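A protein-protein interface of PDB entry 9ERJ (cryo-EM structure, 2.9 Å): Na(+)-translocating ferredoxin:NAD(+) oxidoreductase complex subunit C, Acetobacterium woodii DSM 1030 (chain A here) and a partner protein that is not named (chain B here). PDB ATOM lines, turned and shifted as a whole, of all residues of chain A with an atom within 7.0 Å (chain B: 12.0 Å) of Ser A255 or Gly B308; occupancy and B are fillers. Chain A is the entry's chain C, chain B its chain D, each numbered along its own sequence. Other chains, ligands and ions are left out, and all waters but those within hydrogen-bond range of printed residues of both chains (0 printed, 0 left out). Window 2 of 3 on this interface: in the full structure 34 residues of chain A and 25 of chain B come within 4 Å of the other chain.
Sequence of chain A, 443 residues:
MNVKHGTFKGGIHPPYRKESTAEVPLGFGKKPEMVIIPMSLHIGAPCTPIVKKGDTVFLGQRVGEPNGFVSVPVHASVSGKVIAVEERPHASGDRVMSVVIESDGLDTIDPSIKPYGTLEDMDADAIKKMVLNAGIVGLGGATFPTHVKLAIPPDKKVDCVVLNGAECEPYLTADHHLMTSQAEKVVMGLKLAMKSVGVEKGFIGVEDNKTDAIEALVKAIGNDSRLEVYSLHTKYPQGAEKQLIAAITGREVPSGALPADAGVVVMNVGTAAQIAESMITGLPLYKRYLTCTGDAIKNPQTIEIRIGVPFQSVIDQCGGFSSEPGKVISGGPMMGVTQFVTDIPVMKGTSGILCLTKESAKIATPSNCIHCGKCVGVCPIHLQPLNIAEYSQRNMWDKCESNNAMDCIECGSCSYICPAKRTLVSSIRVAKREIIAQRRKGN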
ATOM      1  N   GLU A 252      35.882 -19.779 -18.967  1.00  0.00           N
ATOM      2  CA  GLU A 252      34.470 -20.120 -19.063  1.00  0.00           C
ATOM      3  C   GLU A 252      33.631 -18.874 -18.827  1.00  0.00           C
ATOM      4  O   GLU A 252      33.860 -18.143 -17.858  1.00  0.00           O
ATOM      5  CB  GLU A 252      34.093 -21.207 -18.052  1.00  0.00           C
ATOM      6  CG  GLU A 252      34.397 -22.621 -18.515  1.00  0.00           C
ATOM      7  CD  GLU A 252      33.712 -23.669 -17.664  1.00  0.00           C
ATOM      8  OE1 GLU A 252      32.985 -23.290 -16.723  1.00  0.00           O
ATOM      9  OE2 GLU A 252      33.902 -24.873 -17.935  1.00  0.00           O
ATOM     10  N   VAL A 253      32.672 -18.636 -19.710  1.00  0.00           N
ATOM     11  CA  VAL A 253      31.745 -17.511 -19.541  1.00  0.00           C
ATOM     12  C   VAL A 253      30.833 -17.794 -18.350  1.00  0.00           C
ATOM     13  O   VAL A 253      30.300 -18.912 -18.237  1.00  0.00           O
ATOM     14  CB  VAL A 253      30.930 -17.298 -20.821  1.00  0.00           C
ATOM     15  CG1 VAL A 253      29.995 -16.111 -20.673  1.00  0.00           C
ATOM     16  CG2 VAL A 253      31.857 -17.103 -22.008  1.00  0.00           C
ATOM     17  N   PRO A 254      30.630 -16.832 -17.437  1.00  0.00           N
ATOM     18  CA  PRO A 254      29.774 -17.085 -16.268  1.00  0.00           C
ATOM     19  C   PRO A 254      28.314 -17.337 -16.619  1.00  0.00           C
ATOM     20  O   PRO A 254      27.918 -17.260 -17.786  1.00  0.00           O
ATOM     21  CB  PRO A 254      29.932 -15.804 -15.439  1.00  0.00           C
ATOM     22  CG  PRO A 254      31.243 -15.241 -15.864  1.00  0.00           C
ATOM     23  CD  PRO A 254      31.343 -15.548 -17.324  1.00  0.00           C
ATOM     24  N   SER A 255      27.503 -17.631 -15.603  1.00  0.00           N
ATOM     25  CA  SER A 255      26.110 -18.031 -15.804  1.00  0.00           C
ATOM     26  C   SER A 255      25.273 -16.792 -16.113  1.00  0.00           C
ATOM     27  O   SER A 255      24.682 -16.157 -15.238  1.00  0.00           O
ATOM     28  CB  SER A 255      25.585 -18.771 -14.581  1.00  0.00           C
ATOM     29  OG  SER A 255      24.401 -19.485 -14.886  1.00  0.00           O
ATOM     30  N   GLY A 256      25.226 -16.448 -17.398  1.00  0.00           N
ATOM     31  CA  GLY A 256      24.426 -15.328 -17.850  1.00  0.00           C
ATOM     32  C   GLY A 256      25.116 -13.993 -17.668  1.00  0.00           C
ATOM     33  O   GLY A 256      24.570 -13.091 -17.027  1.00  0.00           O
ATOM     34  N   ALA A 257      26.320 -13.853 -18.227  1.00  0.00           N
ATOM     35  CA  ALA A 257      27.106 -12.645 -18.042  1.00  0.00           C
ATOM     36  C   ALA A 257      27.791 -12.145 -19.306  1.00  0.00           C
ATOM     37  O   ALA A 257      28.588 -11.205 -19.216  1.00  0.00           O
ATOM     38  CB  ALA A 257      28.166 -12.860 -16.952  1.00  0.00           C
ATOM     39  N   LEU A 258      27.523 -12.757 -20.473  1.00  0.00           N
ATOM     40  CA  LEU A 258      28.032 -12.386 -21.795  1.00  0.00           C
ATOM     41  C   LEU A 258      29.536 -12.628 -21.913  1.00  0.00           C
ATOM     42  O   LEU A 258      30.242 -12.677 -20.898  1.00  0.00           O
ATOM     43  CB  LEU A 258      27.692 -10.924 -22.119  1.00  0.00           C
ATOM     44  CG  LEU A 258      26.454 -10.659 -22.979  1.00  0.00           C
ATOM     45  CD1 LEU A 258      25.208 -11.281 -22.368  1.00  0.00           C
ATOM     46  CD2 LEU A 258      26.262  -9.166 -23.185  1.00  0.00           C
ATOM     47  N   ILE A 381      26.474 -28.391 -22.216  1.00  0.00           N
ATOM     48  CA  ILE A 381      26.293 -27.600 -21.000  1.00  0.00           C
ATOM     49  C   ILE A 381      26.135 -28.484 -19.767  1.00  0.00           C
ATOM     50  O   ILE A 381      26.024 -27.963 -18.648  1.00  0.00           O
ATOM     51  CB  ILE A 381      25.086 -26.650 -21.177  1.00  0.00           C
ATOM     52  CG1 ILE A 381      25.054 -26.094 -22.600  1.00  0.00           C
ATOM     53  CG2 ILE A 381      25.148 -25.470 -20.214  1.00  0.00           C
ATOM     54  CD1 ILE A 381      26.133 -25.066 -22.885  1.00  0.00           C
ATOM     55  N   ASN A 404      17.750 -25.660 -14.108  1.00  0.00           N
ATOM     56  CA  ASN A 404      18.677 -24.868 -14.921  1.00  0.00           C
ATOM     57  C   ASN A 404      18.355 -24.989 -16.413  1.00  0.00           C
ATOM     58  O   ASN A 404      19.152 -25.476 -17.213  1.00  0.00           O
ATOM     59  CB  ASN A 404      20.132 -25.258 -14.635  1.00  0.00           C
ATOM     60  CG  ASN A 404      20.738 -24.456 -13.504  1.00  0.00           C
ATOM     61  OD1 ASN A 404      21.073 -24.999 -12.453  1.00  0.00           O
ATOM     62  ND2 ASN A 404      20.889 -23.156 -13.716  1.00  0.00           N
ATOM     63  N   ASP A 407      19.947 -21.669 -19.237  1.00  0.00           N
ATOM     64  CA  ASP A 407      21.282 -21.567 -19.813  1.00  0.00           C
ATOM     65  C   ASP A 407      21.498 -22.562 -20.947  1.00  0.00           C
ATOM     66  O   ASP A 407      22.641 -22.811 -21.342  1.00  0.00           O
ATOM     67  CB  ASP A 407      22.348 -21.742 -18.731  1.00  0.00           C
ATOM     68  CG  ASP A 407      21.922 -22.695 -17.644  1.00  0.00           C
ATOM     69  OD1 ASP A 407      21.146 -23.621 -17.942  1.00  0.00           O
ATOM     70  OD2 ASP A 407      22.361 -22.515 -16.490  1.00  0.00           O
ATOM     71  N   GLU B 304      26.285 -33.824 -12.136  1.00  0.00           N
ATOM     72  CA  GLU B 304      27.479 -33.184 -12.661  1.00  0.00           C
ATOM     73  C   GLU B 304      27.406 -31.675 -12.436  1.00  0.00           C
ATOM     74  O   GLU B 304      26.450 -31.151 -11.859  1.00  0.00           O
ATOM     75  CB  GLU B 304      27.654 -33.523 -14.141  1.00  0.00           C
ATOM     76  CG  GLU B 304      29.093 -33.778 -14.551  1.00  0.00           C
ATOM     77  CD  GLU B 304      29.240 -34.036 -16.035  1.00  0.00           C
ATOM     78  OE1 GLU B 304      28.228 -34.376 -16.682  1.00  0.00           O
ATOM     79  OE2 GLU B 304      30.367 -33.899 -16.556  1.00  0.00           O
ATOM     80  N   ARG B 305      28.430 -30.963 -12.897  1.00  0.00           N
ATOM     81  CA  ARG B 305      28.537 -29.523 -12.714  1.00  0.00           C
ATOM     82  C   ARG B 305      28.207 -28.818 -14.022  1.00  0.00           C
ATOM     83  O   ARG B 305      28.781 -29.137 -15.067  1.00  0.00           O
ATOM     84  CB  ARG B 305      29.939 -29.137 -12.239  1.00  0.00           C
ATOM     85  CG  ARG B 305      30.008 -27.801 -11.518  1.00  0.00           C
ATOM     86  CD  ARG B 305      31.446 -27.392 -11.254  1.00  0.00           C
ATOM     87  NE  ARG B 305      32.235 -27.342 -12.479  1.00  0.00           N
ATOM     88  CZ  ARG B 305      32.347 -26.272 -13.254  1.00  0.00           C
ATOM     89  NH1 ARG B 305      31.739 -25.137 -12.956  1.00  0.00           N
ATOM     90  NH2 ARG B 305      33.088 -26.344 -14.355  1.00  0.00           N
ATOM     91  N   ILE B 306      27.286 -27.860 -13.954  1.00  0.00           N
ATOM     92  CA  ILE B 306      26.842 -27.142 -15.141  1.00  0.00           C
ATOM     93  C   ILE B 306      27.921 -26.154 -15.582  1.00  0.00           C
ATOM     94  O   ILE B 306      28.619 -25.551 -14.764  1.00  0.00           O
ATOM     95  CB  ILE B 306      25.495 -26.443 -14.867  1.00  0.00           C
ATOM     96  CG1 ILE B 306      24.392 -27.485 -14.697  1.00  0.00           C
ATOM     97  CG2 ILE B 306      25.105 -25.482 -15.980  1.00  0.00           C
ATOM     98  CD1 ILE B 306      23.319 -27.082 -13.725  1.00  0.00           C
ATOM     99  N   TYR B 307      28.079 -26.028 -16.902  1.00  0.00           N
ATOM    100  CA  TYR B 307      29.027 -25.088 -17.492  1.00  0.00           C
ATOM    101  C   TYR B 307      28.731 -23.672 -17.007  1.00  0.00           C
ATOM    102  O   TYR B 307      27.593 -23.201 -17.095  1.00  0.00           O
ATOM    103  CB  TYR B 307      28.945 -25.172 -19.017  1.00  0.00           C
ATOM    104  CG  TYR B 307      29.888 -24.266 -19.791  1.00  0.00           C
ATOM    105  CD1 TYR B 307      29.600 -22.920 -19.988  1.00  0.00           C
ATOM    106  CD2 TYR B 307      31.057 -24.767 -20.345  1.00  0.00           C
ATOM    107  CE1 TYR B 307      30.455 -22.102 -20.689  1.00  0.00           C
ATOM    108  CE2 TYR B 307      31.916 -23.952 -21.057  1.00  0.00           C
ATOM    109  CZ  TYR B 307      31.609 -22.621 -21.225  1.00  0.00           C
ATOM    110  OH  TYR B 307      32.459 -21.805 -21.930  1.00  0.00           O
ATOM    111  N   GLY B 308      29.759 -22.997 -16.497  1.00  0.00           N
ATOM    112  CA  GLY B 308      29.650 -21.627 -16.047  1.00  0.00           C
ATOM    113  C   GLY B 308      29.227 -21.463 -14.604  1.00  0.00           C
ATOM    114  O   GLY B 308      29.447 -20.389 -14.031  1.00  0.00           O
ATOM    115  N   VAL B 309      28.631 -22.490 -14.001  1.00  0.00           N
ATOM    116  CA  VAL B 309      28.202 -22.430 -12.609  1.00  0.00           C
ATOM    117  C   VAL B 309      29.292 -23.018 -11.725  1.00  0.00           C
ATOM    118  O   VAL B 309      29.312 -24.225 -11.464  1.00  0.00           O
ATOM    119  CB  VAL B 309      26.864 -23.164 -12.404  1.00  0.00           C
ATOM    120  CG1 VAL B 309      26.367 -22.973 -10.981  1.00  0.00           C
ATOM    121  CG2 VAL B 309      25.831 -22.671 -13.403  1.00  0.00           C
ATOM    122  N   THR B 310      30.218 -22.173 -11.273  1.00  0.00           N
ATOM    123  CA  THR B 310      31.257 -22.626 -10.356  1.00  0.00           C
ATOM    124  C   THR B 310      31.000 -22.191  -8.919  1.00  0.00           C
ATOM    125  O   THR B 310      31.477 -22.862  -7.996  1.00  0.00           O
ATOM    126  CB  THR B 310      32.630 -22.125 -10.816  1.00  0.00           C
ATOM    127  OG1 THR B 310      33.647 -22.650  -9.953  1.00  0.00           O
ATOM    128  CG2 THR B 310      32.692 -20.603 -10.804  1.00  0.00           C
ATOM    129  N   LYS B 311      30.230 -21.116  -8.719  1.00  0.00           N
ATOM    130  CA  LYS B 311      29.941 -20.515  -7.418  1.00  0.00           C
ATOM    131  C   LYS B 311      31.180 -20.389  -6.538  1.00  0.00           C
ATOM    132  O   LYS B 311      32.274 -20.100  -7.031  1.00  0.00           O
ATOM    133  CB  LYS B 311      28.865 -21.325  -6.685  1.00  0.00           C
ATOM    134  CG  LYS B 311      27.826 -21.963  -7.595  1.00  0.00           C
ATOM    135  CD  LYS B 311      27.231 -23.212  -6.966  1.00  0.00           C
ATOM    136  CE  LYS B 311      28.306 -24.235  -6.636  1.00  0.00           C
ATOM    137  NZ  LYS B 311      29.084 -24.642  -7.838  1.00  0.00           N
ATOM    138  N   ILE B 312      31.011 -20.598  -5.233  1.00  0.00           N
ATOM    139  CA  ILE B 312      32.129 -20.638  -4.297  1.00  0.00           C
ATOM    140  C   ILE B 312      32.065 -21.938  -3.508  1.00  0.00           C
ATOM    141  O   ILE B 312      33.048 -22.684  -3.434  1.00  0.00           O
ATOM    142  CB  ILE B 312      32.136 -19.423  -3.348  1.00  0.00           C
ATOM    143  CG1 ILE B 312      31.808 -18.127  -4.097  1.00  0.00           C
ATOM    144  CG2 ILE B 312      33.479 -19.310  -2.641  1.00  0.00           C
ATOM    145  CD1 ILE B 312      30.415 -17.593  -3.827  1.00  0.00           C
ATOM    146  N   LYS B 313      30.904 -22.218  -2.914  1.00  0.00           N
ATOM    147  CA  LYS B 313      30.754 -23.371  -2.035  1.00  0.00           C
ATOM    148  C   LYS B 313      29.311 -23.870  -2.151  1.00  0.00           C
ATOM    149  O   LYS B 313      28.618 -23.537  -3.118  1.00  0.00           O
ATOM    150  CB  LYS B 313      31.152 -22.983  -0.602  1.00  0.00           C
ATOM    151  CG  LYS B 313      31.440 -24.137   0.365  1.00  0.00           C
ATOM    152  CD  LYS B 313      32.666 -24.921  -0.075  1.00  0.00           C
ATOM    153  CE  LYS B 313      32.448 -26.418   0.079  1.00  0.00           C
ATOM    154  NZ  LYS B 313      31.794 -27.005  -1.124  1.00  0.00           N
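Among the printed residues, merely in contact across the chains: Asn A404 with Ile B306 (3.3 Å), Val A253 with Gly B308 (3.5 Å), Ile A381 with Ile B306 (3.7 Å), Ser A255 with Gly B308 (3.7 Å), Glu A252 with Tyr B307 (3.7 Å), Ser A255 with Val B309 (3.8 Å) and Val A253 with Tyr B307 (3.9 Å).
Of the 10 printed residues of chain B, 5 touch a printed residue of chain A. Printed residues of chain B that touch a printed residue of chain A: Arg B305, Ile B306, Tyr B307, Gly B308 and Val B309. Hydrophobic or aromatic side chains of chain B that line the printed part of chain A: Ile B306, Tyr B307 and Val B309. Hydrophobic or aromatic side chains of chain A that line the printed part of chain B: Ile A381. Among the printed residues, 10 pairs touch across the chains. Among the printed residues, Asp or Glu carboxylates within 4 Å of a Lys or Arg side-chain nitrogen of the other chain: Glu A252 with Arg B305 (3.9 Å).
OD2 of Asp A407 is in hydrogen-bond range of ND2 of Asn A404. The guanidinium group of Arg B305 sits at hydrogen-bond distance from the backbone carbonyl oxygen of Val B309, 3.0 Å away.
Printed residues of chain B within 4 Å of Glu A252: Arg B305, Tyr B307 and Gly B308. Val A253 touches two residues of chain B. Ser A255 touches two residues of chain B. Gly A256 touches none of the printed residues of chain B. No residue of chain B comes within 4 Å of Ala A257. Of the printed residues of chain B, Ile A381 touches Ile B306 and Tyr B307. Printed residues of chain B within 4 Å of Asn A404: Ile B306 (3.3 Å). No residue of chain B comes within 4 Å of Asp A407. Of the printed residues of chain A, Arg B305 touches Glu A252. Of the printed residues of chain A, Tyr B307 touches Glu A252 (3.7 Å), Val A253 (3.9 Å) and Ile A381 (3.3 Å). Of the printed residues of chain A, Val B309 touches Ser A255 (3.8 Å). The nearest printed residue of chain A that does not touch Val B309 is Asp A407 (4.6 Å).
The guanidinium group (NH2) of Arg B305 is in salt-bridge range of the side-chain carboxylate (OE1) of Glu A252 (3.9 Å). The side-chain carboxylate (OE1) of Glu A252 lies within hydrogen-bond range of the backbone NH (N) of Gly B308 (3.2 Å). N of Tyr B307 sits at hydrogen-bond distance from O of Ile A381.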
